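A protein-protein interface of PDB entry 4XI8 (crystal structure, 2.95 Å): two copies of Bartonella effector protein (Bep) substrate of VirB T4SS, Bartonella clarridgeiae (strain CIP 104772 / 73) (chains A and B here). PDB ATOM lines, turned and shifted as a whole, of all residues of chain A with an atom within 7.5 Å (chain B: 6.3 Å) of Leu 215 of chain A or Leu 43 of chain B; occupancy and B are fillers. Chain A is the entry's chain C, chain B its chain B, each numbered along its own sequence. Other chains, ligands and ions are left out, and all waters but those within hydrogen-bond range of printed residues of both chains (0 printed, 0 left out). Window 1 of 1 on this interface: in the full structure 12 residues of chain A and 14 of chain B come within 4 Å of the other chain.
Hydrophobic or aromatic side chains of chain B within 4 Å of the printed part of chain A: Tyr 40, Leu 43, Met 46 and Leu 47.
Along chain B the printed residues that touch a printed residue of chain A span positions 40 to 47.
Of the 22 printed residues of chain A, 8 touch a printed residue of chain B.
Among the printed residues, 11 pairs touch across the chains.
Among the printed residues, no Asp or Glu carboxylate lies within 4 Å of a Lys or Arg side-chain nitrogen of the other chain.
Of chain B, only Leu 43 (3.9 Å) comes within 4 Å of Leu 215 of chain A.
Of the printed residues of chain A, Leu 43 of chain B touches Asp 205 (3.5 Å), Lys 211 (3.99 Å), Ile 214 (3.7 Å) and Leu 215 (3.9 Å).
Of the printed residues of chain B, Ile 214 of chain A touches Leu 43 (3.7 Å) and Leu 47 (3.9 Å).
Printed residues of chain B within 4 Å of Glu 204 of chain A: Tyr 40.
Printed residues of chain A within 4 Å of Met 46 of chain B: Phe 218 (3.8 Å).
Asn 208 of chain A touches none of the printed residues of chain B.
The nearest printed residue of chain B that does not touch Leu 215 of chain A is Ala 39 of chain B (6.7 Å).
The nearest printed residue of chain B that does not touch Phe 218 of chain A is Leu 43 of chain B (6.4 Å).
The side-chain hydroxyl (OH) of Tyr 40 of chain B is in hydrogen-bond range of the side-chain carboxylate (OE1) of Glu 204 of chain A, 3.2 Å away.
The side-chain amino group (NZ) of Lys 211 of chain A lies within hydrogen-bond range of the side-chain amide oxygen (OE1) of Gln 44 of chain B (3.1 Å).
No position is printed for both chains.
Of the 11 pairs that touch across the chains among the printed residues, none has its exchanged pair printed and touching as well.
The backbone carbonyl oxygen of Gln 44 of chain B lies close to the side-chain amide oxygen of Asn 48 of chain B, at 2.8 Å.
The guanidinium group (NH2) of Arg 176 of chain A sits at hydrogen-bond distance from the backbone carbonyl oxygen (O) of His 201 of chain A, 3.3 Å away.
The guanidinium group (NH2) of Arg 176 of chain A lies within salt-bridge range of the side-chain carboxylate (OD2) of Asp 205 of chain A.
The side-chain carboxylate (OE1) of Glu 204 of chain A lies within salt-bridge range of the side-chain amino group (NZ) of Lys 211 of chain A (2.7 Å).
The side-chain amino group (NZ) of Lys 211 of chain A is in salt-bridge range of the side-chain carboxylate (OD1) of Asp 205 of chain A (3.3 Å).
The side-chain amide oxygen (OD1) of Asn 208 of chain A sits close to the backbone NH (N) of Glu 210 of chain A (3.2 Å).
Among the printed residues, pairs that only touch across the chains: His 201 of chain A with Tyr 40 of chain B, Asp 205 of chain A with Tyr 40 of chain B, Asp 205 of chain A with Leu 43 of chain B, Glu 210 of chain A with Leu 47 of chain B, Lys 211 of chain A with Leu 43 of chain B, Ile 214 of chain A with Leu 43 of chain B, Ile 214 of chain A with Leu 47 of chain B, Leu 215 of chain A with Leu 43 of chain B and Phe 218 of chain A with Met 46 of chain B.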
ATOM      1  N   ASP A 168     -26.695  -8.282  -0.567  1.00  0.00           N
ATOM      2  CA  ASP A 168     -25.317  -8.754  -0.643  1.00  0.00           C
ATOM      3  C   ASP A 168     -25.075  -9.846   0.400  1.00  0.00           C
ATOM      4  O   ASP A 168     -24.756  -9.554   1.553  1.00  0.00           O
ATOM      5  CB  ASP A 168     -24.342  -7.592  -0.437  1.00  0.00           C
ATOM      6  CG  ASP A 168     -22.962  -7.879  -0.995  1.00  0.00           C
ATOM      7  OD1 ASP A 168     -22.602  -9.068  -1.123  1.00  0.00           O
ATOM      8  OD2 ASP A 168     -22.236  -6.912  -1.307  1.00  0.00           O
ATOM      9  N   VAL A 171     -21.443 -10.918   2.821  1.00  0.00           N
ATOM     10  CA  VAL A 171     -20.988 -10.446   4.124  1.00  0.00           C
ATOM     11  C   VAL A 171     -21.691 -11.154   5.282  1.00  0.00           C
ATOM     12  O   VAL A 171     -21.700 -10.655   6.407  1.00  0.00           O
ATOM     13  CB  VAL A 171     -21.189  -8.924   4.271  1.00  0.00           C
ATOM     14  CG1 VAL A 171     -20.252  -8.174   3.336  1.00  0.00           C
ATOM     15  CG2 VAL A 171     -22.633  -8.549   3.998  1.00  0.00           C
ATOM     16  N   VAL A 172     -22.277 -12.315   5.003  1.00  0.00           N
ATOM     17  CA  VAL A 172     -22.919 -13.111   6.045  1.00  0.00           C
ATOM     18  C   VAL A 172     -22.097 -14.343   6.398  1.00  0.00           C
ATOM     19  O   VAL A 172     -21.770 -15.152   5.530  1.00  0.00           O
ATOM     20  CB  VAL A 172     -24.326 -13.577   5.625  1.00  0.00           C
ATOM     21  CG1 VAL A 172     -25.033 -14.249   6.794  1.00  0.00           C
ATOM     22  CG2 VAL A 172     -25.140 -12.413   5.108  1.00  0.00           C
ATOM     23  N   ARG A 176     -23.930 -16.839  11.641  1.00  0.00           N
ATOM     24  CA  ARG A 176     -25.027 -15.885  11.771  1.00  0.00           C
ATOM     25  C   ARG A 176     -26.288 -16.404  11.092  1.00  0.00           C
ATOM     26  O   ARG A 176     -27.386 -16.300  11.640  1.00  0.00           O
ATOM     27  CB  ARG A 176     -24.639 -14.527  11.184  1.00  0.00           C
ATOM     28  CG  ARG A 176     -25.719 -13.468  11.337  1.00  0.00           C
ATOM     29  CD  ARG A 176     -25.289 -12.134  10.756  1.00  0.00           C
ATOM     30  NE  ARG A 176     -26.312 -11.108  10.942  1.00  0.00           N
ATOM     31  CZ  ARG A 176     -26.186  -9.847  10.543  1.00  0.00           C
ATOM     32  NH1 ARG A 176     -25.080  -9.450   9.928  1.00  0.00           N
ATOM     33  NH2 ARG A 176     -27.167  -8.980  10.757  1.00  0.00           N
ATOM     34  N   HIS A 201     -32.959  -8.581  11.204  1.00  0.00           N
ATOM     35  CA  HIS A 201     -31.698  -7.873  11.394  1.00  0.00           C
ATOM     36  C   HIS A 201     -30.696  -8.224  10.303  1.00  0.00           C
ATOM     37  O   HIS A 201     -29.928  -7.372   9.856  1.00  0.00           O
ATOM     38  CB  HIS A 201     -31.098  -8.192  12.765  1.00  0.00           C
ATOM     39  CG  HIS A 201     -31.848  -7.586  13.910  1.00  0.00           C
ATOM     40  ND1 HIS A 201     -31.512  -7.824  15.225  1.00  0.00           N
ATOM     41  CD2 HIS A 201     -32.910  -6.748  13.938  1.00  0.00           C
ATOM     42  CE1 HIS A 201     -32.338  -7.159  16.016  1.00  0.00           C
ATOM     43  NE2 HIS A 201     -33.196  -6.499  15.258  1.00  0.00           N
ATOM     44  N   LEU A 202     -30.707  -9.486   9.884  1.00  0.00           N
ATOM     45  CA  LEU A 202     -29.802  -9.955   8.844  1.00  0.00           C
ATOM     46  C   LEU A 202     -30.089  -9.236   7.532  1.00  0.00           C
ATOM     47  O   LEU A 202     -29.219  -8.570   6.976  1.00  0.00           O
ATOM     48  CB  LEU A 202     -29.930 -11.473   8.667  1.00  0.00           C
ATOM     49  CG  LEU A 202     -28.866 -12.216   7.852  1.00  0.00           C
ATOM     50  CD1 LEU A 202     -28.719 -13.639   8.365  1.00  0.00           C
ATOM     51  CD2 LEU A 202     -29.196 -12.227   6.364  1.00  0.00           C
ATOM     52  N   GLU A 204     -31.813  -6.646   6.955  1.00  0.00           N
ATOM     53  CA  GLU A 204     -31.763  -5.192   7.060  1.00  0.00           C
ATOM     54  C   GLU A 204     -30.337  -4.697   6.843  1.00  0.00           C
ATOM     55  O   GLU A 204     -30.117  -3.673   6.197  1.00  0.00           O
ATOM     56  CB  GLU A 204     -32.295  -4.729   8.420  1.00  0.00           C
ATOM     57  CG  GLU A 204     -32.508  -3.222   8.542  1.00  0.00           C
ATOM     58  CD  GLU A 204     -31.241  -2.470   8.905  1.00  0.00           C
ATOM     59  OE1 GLU A 204     -30.363  -3.066   9.562  1.00  0.00           O
ATOM     60  OE2 GLU A 204     -31.123  -1.285   8.530  1.00  0.00           O
ATOM     61  N   ASP A 205     -29.373  -5.432   7.388  1.00  0.00           N
ATOM     62  CA  ASP A 205     -27.963  -5.121   7.187  1.00  0.00           C
ATOM     63  C   ASP A 205     -27.568  -5.388   5.741  1.00  0.00           C
ATOM     64  O   ASP A 205     -26.794  -4.641   5.142  1.00  0.00           O
ATOM     65  CB  ASP A 205     -27.084  -5.944   8.131  1.00  0.00           C
ATOM     66  CG  ASP A 205     -27.312  -5.601   9.590  1.00  0.00           C
ATOM     67  OD1 ASP A 205     -27.942  -4.560   9.868  1.00  0.00           O
ATOM     68  OD2 ASP A 205     -26.858  -6.375  10.459  1.00  0.00           O
ATOM     69  N   ILE A 206     -28.118  -6.464   5.190  1.00  0.00           N
ATOM     70  CA  ILE A 206     -27.797  -6.911   3.841  1.00  0.00           C
ATOM     71  C   ILE A 206     -28.317  -5.950   2.772  1.00  0.00           C
ATOM     72  O   ILE A 206     -27.648  -5.707   1.766  1.00  0.00           O
ATOM     73  CB  ILE A 206     -28.361  -8.330   3.597  1.00  0.00           C
ATOM     74  CG1 ILE A 206     -27.614  -9.340   4.461  1.00  0.00           C
ATOM     75  CG2 ILE A 206     -28.245  -8.728   2.148  1.00  0.00           C
ATOM     76  CD1 ILE A 206     -26.129  -9.098   4.508  1.00  0.00           C
ATOM     77  N   ASN A 208     -28.649  -2.876   3.155  1.00  0.00           N
ATOM     78  CA  ASN A 208     -28.066  -1.570   3.434  1.00  0.00           C
ATOM     79  C   ASN A 208     -26.620  -1.501   2.946  1.00  0.00           C
ATOM     80  O   ASN A 208     -25.719  -2.032   3.594  1.00  0.00           O
ATOM     81  CB  ASN A 208     -28.138  -1.264   4.933  1.00  0.00           C
ATOM     82  CG  ASN A 208     -27.849   0.193   5.253  1.00  0.00           C
ATOM     83  OD1 ASN A 208     -27.264   0.919   4.448  1.00  0.00           O
ATOM     84  ND2 ASN A 208     -28.263   0.627   6.437  1.00  0.00           N
ATOM     85  N   PRO A 209     -26.401  -0.841   1.796  1.00  0.00           N
ATOM     86  CA  PRO A 209     -25.086  -0.709   1.157  1.00  0.00           C
ATOM     87  C   PRO A 209     -24.030  -0.125   2.092  1.00  0.00           C
ATOM     88  O   PRO A 209     -22.877  -0.555   2.067  1.00  0.00           O
ATOM     89  CB  PRO A 209     -25.360   0.243  -0.011  1.00  0.00           C
ATOM     90  CG  PRO A 209     -26.802   0.053  -0.315  1.00  0.00           C
ATOM     91  CD  PRO A 209     -27.460  -0.181   1.011  1.00  0.00           C
ATOM     92  N   GLU A 210     -24.433   0.848   2.903  1.00  0.00           N
ATOM     93  CA  GLU A 210     -23.527   1.493   3.847  1.00  0.00           C
ATOM     94  C   GLU A 210     -23.064   0.517   4.928  1.00  0.00           C
ATOM     95  O   GLU A 210     -21.894   0.515   5.309  1.00  0.00           O
ATOM     96  CB  GLU A 210     -24.202   2.713   4.478  1.00  0.00           C
ATOM     97  CG  GLU A 210     -24.489   3.830   3.481  1.00  0.00           C
ATOM     98  CD  GLU A 210     -24.680   5.182   4.143  1.00  0.00           C
ATOM     99  OE1 GLU A 210     -24.777   5.233   5.386  1.00  0.00           O
ATOM    100  OE2 GLU A 210     -24.732   6.197   3.417  1.00  0.00           O
ATOM    101  N   LYS A 211     -23.983  -0.312   5.415  1.00  0.00           N
ATOM    102  CA  LYS A 211     -23.655  -1.302   6.438  1.00  0.00           C
ATOM    103  C   LYS A 211     -22.807  -2.439   5.877  1.00  0.00           C
ATOM    104  O   LYS A 211     -21.954  -2.988   6.574  1.00  0.00           O
ATOM    105  CB  LYS A 211     -24.925  -1.872   7.071  1.00  0.00           C
ATOM    106  CG  LYS A 211     -25.654  -0.906   7.986  1.00  0.00           C
ATOM    107  CD  LYS A 211     -26.774  -1.610   8.732  1.00  0.00           C
ATOM    108  CE  LYS A 211     -27.443  -0.677   9.725  1.00  0.00           C
ATOM    109  NZ  LYS A 211     -28.481  -1.373  10.533  1.00  0.00           N
ATOM    110  N   VAL A 212     -23.052  -2.793   4.619  1.00  0.00           N
ATOM    111  CA  VAL A 212     -22.284  -3.843   3.958  1.00  0.00           C
ATOM    112  C   VAL A 212     -20.817  -3.436   3.853  1.00  0.00           C
ATOM    113  O   VAL A 212     -19.918  -4.258   4.042  1.00  0.00           O
ATOM    114  CB  VAL A 212     -22.843  -4.151   2.551  1.00  0.00           C
ATOM    115  CG1 VAL A 212     -21.929  -5.111   1.805  1.00  0.00           C
ATOM    116  CG2 VAL A 212     -24.246  -4.726   2.655  1.00  0.00           C
ATOM    117  N   GLY A 213     -20.584  -2.158   3.571  1.00  0.00           N
ATOM    118  CA  GLY A 213     -19.235  -1.629   3.488  1.00  0.00           C
ATOM    119  C   GLY A 213     -18.506  -1.690   4.816  1.00  0.00           C
ATOM    120  O   GLY A 213     -17.311  -1.978   4.865  1.00  0.00           O
ATOM    121  N   ILE A 214     -19.229  -1.414   5.897  1.00  0.00           N
ATOM    122  CA  ILE A 214     -18.656  -1.459   7.238  1.00  0.00           C
ATOM    123  C   ILE A 214     -18.304  -2.891   7.631  1.00  0.00           C
ATOM    124  O   ILE A 214     -17.260  -3.141   8.235  1.00  0.00           O
ATOM    125  CB  ILE A 214     -19.621  -0.858   8.281  1.00  0.00           C
ATOM    126  CG1 ILE A 214     -19.933   0.601   7.940  1.00  0.00           C
ATOM    127  CG2 ILE A 214     -19.038  -0.965   9.684  1.00  0.00           C
ATOM    128  CD1 ILE A 214     -20.838   1.285   8.941  1.00  0.00           C
ATOM    129  N   LEU A 215     -19.178  -3.829   7.278  1.00  0.00           N
ATOM    130  CA  LEU A 215     -18.957  -5.243   7.568  1.00  0.00           C
ATOM    131  C   LEU A 215     -17.706  -5.769   6.867  1.00  0.00           C
ATOM    132  O   LEU A 215     -17.014  -6.645   7.385  1.00  0.00           O
ATOM    133  CB  LEU A 215     -20.175  -6.073   7.158  1.00  0.00           C
ATOM    134  CG  LEU A 215     -21.413  -5.953   8.052  1.00  0.00           C
ATOM    135  CD1 LEU A 215     -22.551  -6.803   7.509  1.00  0.00           C
ATOM    136  CD2 LEU A 215     -21.086  -6.343   9.486  1.00  0.00           C
ATOM    137  N   LYS A 216     -17.427  -5.229   5.684  1.00  0.00           N
ATOM    138  CA  LYS A 216     -16.261  -5.626   4.901  1.00  0.00           C
ATOM    139  C   LYS A 216     -14.951  -5.176   5.548  1.00  0.00           C
ATOM    140  O   LYS A 216     -13.893  -5.746   5.286  1.00  0.00           O
ATOM    141  CB  LYS A 216     -16.360  -5.064   3.481  1.00  0.00           C
ATOM    142  N   GLU A 217     -15.031  -4.153   6.393  1.00  0.00           N
ATOM    143  CA  GLU A 217     -13.851  -3.597   7.050  1.00  0.00           C
ATOM    144  C   GLU A 217     -13.443  -4.391   8.288  1.00  0.00           C
ATOM    145  O   GLU A 217     -12.432  -4.085   8.920  1.00  0.00           O
ATOM    146  CB  GLU A 217     -14.090  -2.136   7.437  1.00  0.00           C
ATOM    147  CG  GLU A 217     -14.431  -1.224   6.273  1.00  0.00           C
ATOM    148  CD  GLU A 217     -14.652   0.210   6.710  1.00  0.00           C
ATOM    149  OE1 GLU A 217     -15.242   0.988   5.930  1.00  0.00           O
ATOM    150  OE2 GLU A 217     -14.231   0.562   7.831  1.00  0.00           O
ATOM    151  N   PHE A 218     -14.227  -5.406   8.633  1.00  0.00           N
ATOM    152  CA  PHE A 218     -13.935  -6.218   9.809  1.00  0.00           C
ATOM    153  C   PHE A 218     -13.757  -7.691   9.456  1.00  0.00           C
ATOM    154  O   PHE A 218     -13.624  -8.538  10.340  1.00  0.00           O
ATOM    155  CB  PHE A 218     -15.043  -6.057  10.850  1.00  0.00           C
ATOM    156  CG  PHE A 218     -15.057  -4.710  11.512  1.00  0.00           C
ATOM    157  CD1 PHE A 218     -14.317  -4.481  12.661  1.00  0.00           C
ATOM    158  CD2 PHE A 218     -15.802  -3.671  10.983  1.00  0.00           C
ATOM    159  CE1 PHE A 218     -14.324  -3.240  13.271  1.00  0.00           C
ATOM    160  CE2 PHE A 218     -15.814  -2.428  11.589  1.00  0.00           C
ATOM    161  CZ  PHE A 218     -15.075  -2.213  12.733  1.00  0.00           C
ATOM    162  N   MET A 219     -13.753  -7.992   8.162  1.00  0.00           N
ATOM    163  CA  MET A 219     -13.507  -9.350   7.697  1.00  0.00           C
ATOM    164  C   MET A 219     -12.012  -9.655   7.741  1.00  0.00           C
ATOM    165  O   MET A 219     -11.313  -9.526   6.736  1.00  0.00           O
ATOM    166  CB  MET A 219     -14.048  -9.545   6.279  1.00  0.00           C
ATOM    167  N   ILE A 220     -11.530 -10.052   8.915  1.00  0.00           N
ATOM    168  CA  ILE A 220     -10.113 -10.334   9.117  1.00  0.00           C
ATOM    169  C   ILE A 220      -9.631 -11.489   8.245  1.00  0.00           C
ATOM    170  O   ILE A 220      -8.505 -11.474   7.746  1.00  0.00           O
ATOM    171  CB  ILE A 220      -9.810 -10.664  10.590  1.00  0.00           C
ATOM    172  N   CYS B  38     -26.425  -7.495  20.284  1.00  0.00           N
ATOM    173  CA  CYS B  38     -25.323  -6.574  20.539  1.00  0.00           C
ATOM    174  C   CYS B  38     -24.618  -6.161  19.251  1.00  0.00           C
ATOM    175  O   CYS B  38     -24.297  -4.990  19.057  1.00  0.00           O
ATOM    176  CB  CYS B  38     -24.317  -7.202  21.507  1.00  0.00           C
ATOM    177  SG  CYS B  38     -22.957  -6.110  21.985  1.00  0.00           S
ATOM    178  N   ALA B  39     -24.381  -7.132  18.375  1.00  0.00           N
ATOM    179  CA  ALA B  39     -23.682  -6.884  17.119  1.00  0.00           C
ATOM    180  C   ALA B  39     -24.492  -5.993  16.184  1.00  0.00           C
ATOM    181  O   ALA B  39     -23.932  -5.185  15.443  1.00  0.00           O
ATOM    182  CB  ALA B  39     -23.348  -8.200  16.434  1.00  0.00           C
ATOM    183  N   TYR B  40     -25.813  -6.141  16.224  1.00  0.00           N
ATOM    184  CA  TYR B  40     -26.694  -5.355  15.370  1.00  0.00           C
ATOM    185  C   TYR B  40     -26.677  -3.880  15.759  1.00  0.00           C
ATOM    186  O   TYR B  40     -26.580  -3.003  14.901  1.00  0.00           O
ATOM    187  CB  TYR B  40     -28.124  -5.898  15.429  1.00  0.00           C
ATOM    188  CG  TYR B  40     -29.117  -5.093  14.621  1.00  0.00           C
ATOM    189  CD1 TYR B  40     -29.181  -5.218  13.239  1.00  0.00           C
ATOM    190  CD2 TYR B  40     -29.991  -4.210  15.240  1.00  0.00           C
ATOM    191  CE1 TYR B  40     -30.088  -4.485  12.497  1.00  0.00           C
ATOM    192  CE2 TYR B  40     -30.901  -3.472  14.507  1.00  0.00           C
ATOM    193  CZ  TYR B  40     -30.946  -3.614  13.136  1.00  0.00           C
ATOM    194  OH  TYR B  40     -31.850  -2.881  12.403  1.00  0.00           O
ATOM    195  N   ASP B  41     -26.773  -3.614  17.057  1.00  0.00           N
ATOM    196  CA  ASP B  41     -26.752  -2.246  17.561  1.00  0.00           C
ATOM    197  C   ASP B  41     -25.369  -1.623  17.419  1.00  0.00           C
ATOM    198  O   ASP B  41     -25.241  -0.415  17.218  1.00  0.00           O
ATOM    199  CB  ASP B  41     -27.203  -2.210  19.022  1.00  0.00           C
ATOM    200  CG  ASP B  41     -28.695  -2.424  19.172  1.00  0.00           C
ATOM    201  OD1 ASP B  41     -29.413  -2.345  18.153  1.00  0.00           O
ATOM    202  OD2 ASP B  41     -29.150  -2.675  20.306  1.00  0.00           O
ATOM    203  N   LEU B  42     -24.335  -2.452  17.528  1.00  0.00           N
ATOM    204  CA  LEU B  42     -22.963  -1.983  17.373  1.00  0.00           C
ATOM    205  C   LEU B  42     -22.715  -1.531  15.938  1.00  0.00           C
ATOM    206  O   LEU B  42     -22.025  -0.541  15.701  1.00  0.00           O
ATOM    207  CB  LEU B  42     -21.967  -3.077  17.764  1.00  0.00           C
ATOM    208  CG  LEU B  42     -20.507  -2.635  17.877  1.00  0.00           C
ATOM    209  CD1 LEU B  42     -20.340  -1.609  18.984  1.00  0.00           C
ATOM    210  CD2 LEU B  42     -19.596  -3.829  18.110  1.00  0.00           C
ATOM    211  N   LEU B  43     -23.285  -2.265  14.987  1.00  0.00           N
ATOM    212  CA  LEU B  43     -23.147  -1.930  13.574  1.00  0.00           C
ATOM    213  C   LEU B  43     -23.880  -0.635  13.249  1.00  0.00           C
ATOM    214  O   LEU B  43     -23.396   0.184  12.467  1.00  0.00           O
ATOM    215  CB  LEU B  43     -23.676  -3.070  12.700  1.00  0.00           C
ATOM    216  CG  LEU B  43     -23.614  -2.865  11.185  1.00  0.00           C
ATOM    217  CD1 LEU B  43     -22.194  -2.563  10.738  1.00  0.00           C
ATOM    218  CD2 LEU B  43     -24.160  -4.085  10.458  1.00  0.00           C
ATOM    219  N   GLN B  44     -25.048  -0.452  13.857  1.00  0.00           N
ATOM    220  CA  GLN B  44     -25.822   0.769  13.676  1.00  0.00           C
ATOM    221  C   GLN B  44     -25.098   1.969  14.274  1.00  0.00           C
ATOM    222  O   GLN B  44     -25.092   3.055  13.692  1.00  0.00           O
ATOM    223  CB  GLN B  44     -27.210   0.627  14.303  1.00  0.00           C
ATOM    224  CG  GLN B  44     -28.055   1.892  14.228  1.00  0.00           C
ATOM    225  CD  GLN B  44     -28.491   2.229  12.816  1.00  0.00           C
ATOM    226  OE1 GLN B  44     -28.450   1.387  11.922  1.00  0.00           O
ATOM    227  NE2 GLN B  44     -28.907   3.473  12.609  1.00  0.00           N
ATOM    228  N   ALA B  45     -24.477   1.760  15.430  1.00  0.00           N
ATOM    229  CA  ALA B  45     -23.770   2.827  16.128  1.00  0.00           C
ATOM    230  C   ALA B  45     -22.582   3.320  15.312  1.00  0.00           C
ATOM    231  O   ALA B  45     -22.299   4.518  15.271  1.00  0.00           O
ATOM    232  CB  ALA B  45     -23.315   2.353  17.496  1.00  0.00           C
ATOM    233  N   MET B  46     -21.888   2.389  14.666  1.00  0.00           N
ATOM    234  CA  MET B  46     -20.752   2.728  13.817  1.00  0.00           C
ATOM    235  C   MET B  46     -21.197   3.546  12.610  1.00  0.00           C
ATOM    236  O   MET B  46     -20.485   4.444  12.159  1.00  0.00           O
ATOM    237  CB  MET B  46     -20.033   1.463  13.348  1.00  0.00           C
ATOM    238  CG  MET B  46     -19.329   0.697  14.448  1.00  0.00           C
ATOM    239  SD  MET B  46     -18.457  -0.745  13.811  1.00  0.00           S
ATOM    240  CE  MET B  46     -17.741  -1.393  15.317  1.00  0.00           C
ATOM    241  N   LEU B  47     -22.378   3.224  12.093  1.00  0.00           N
ATOM    242  CA  LEU B  47     -22.930   3.923  10.941  1.00  0.00           C
ATOM    243  C   LEU B  47     -23.242   5.384  11.256  1.00  0.00           C
ATOM    244  O   LEU B  47     -22.950   6.274  10.458  1.00  0.00           O
ATOM    245  CB  LEU B  47     -24.192   3.213  10.447  1.00  0.00           C
ATOM    246  CG  LEU B  47     -24.839   3.800   9.194  1.00  0.00           C
ATOM    247  CD1 LEU B  47     -23.859   3.749   8.037  1.00  0.00           C
ATOM    248  CD2 LEU B  47     -26.122   3.061   8.850  1.00  0.00           C
ATOM    249  N   ASN B  48     -23.835   5.625  12.422  1.00  0.00           N
ATOM    250  CA  ASN B  48     -24.164   6.984  12.840  1.00  0.00           C
ATOM    251  C   ASN B  48     -22.928   7.805  13.198  1.00  0.00           C
ATOM    252  O   ASN B  48     -22.911   9.022  13.021  1.00  0.00           O
ATOM    253  CB  ASN B  48     -25.133   6.966  14.025  1.00  0.00           C
ATOM    254  CG  ASN B  48     -26.485   6.378  13.665  1.00  0.00           C
ATOM    255  OD1 ASN B  48     -26.783   5.229  13.986  1.00  0.00           O
ATOM    256  ND2 ASN B  48     -27.312   7.171  12.992  1.00  0.00           N
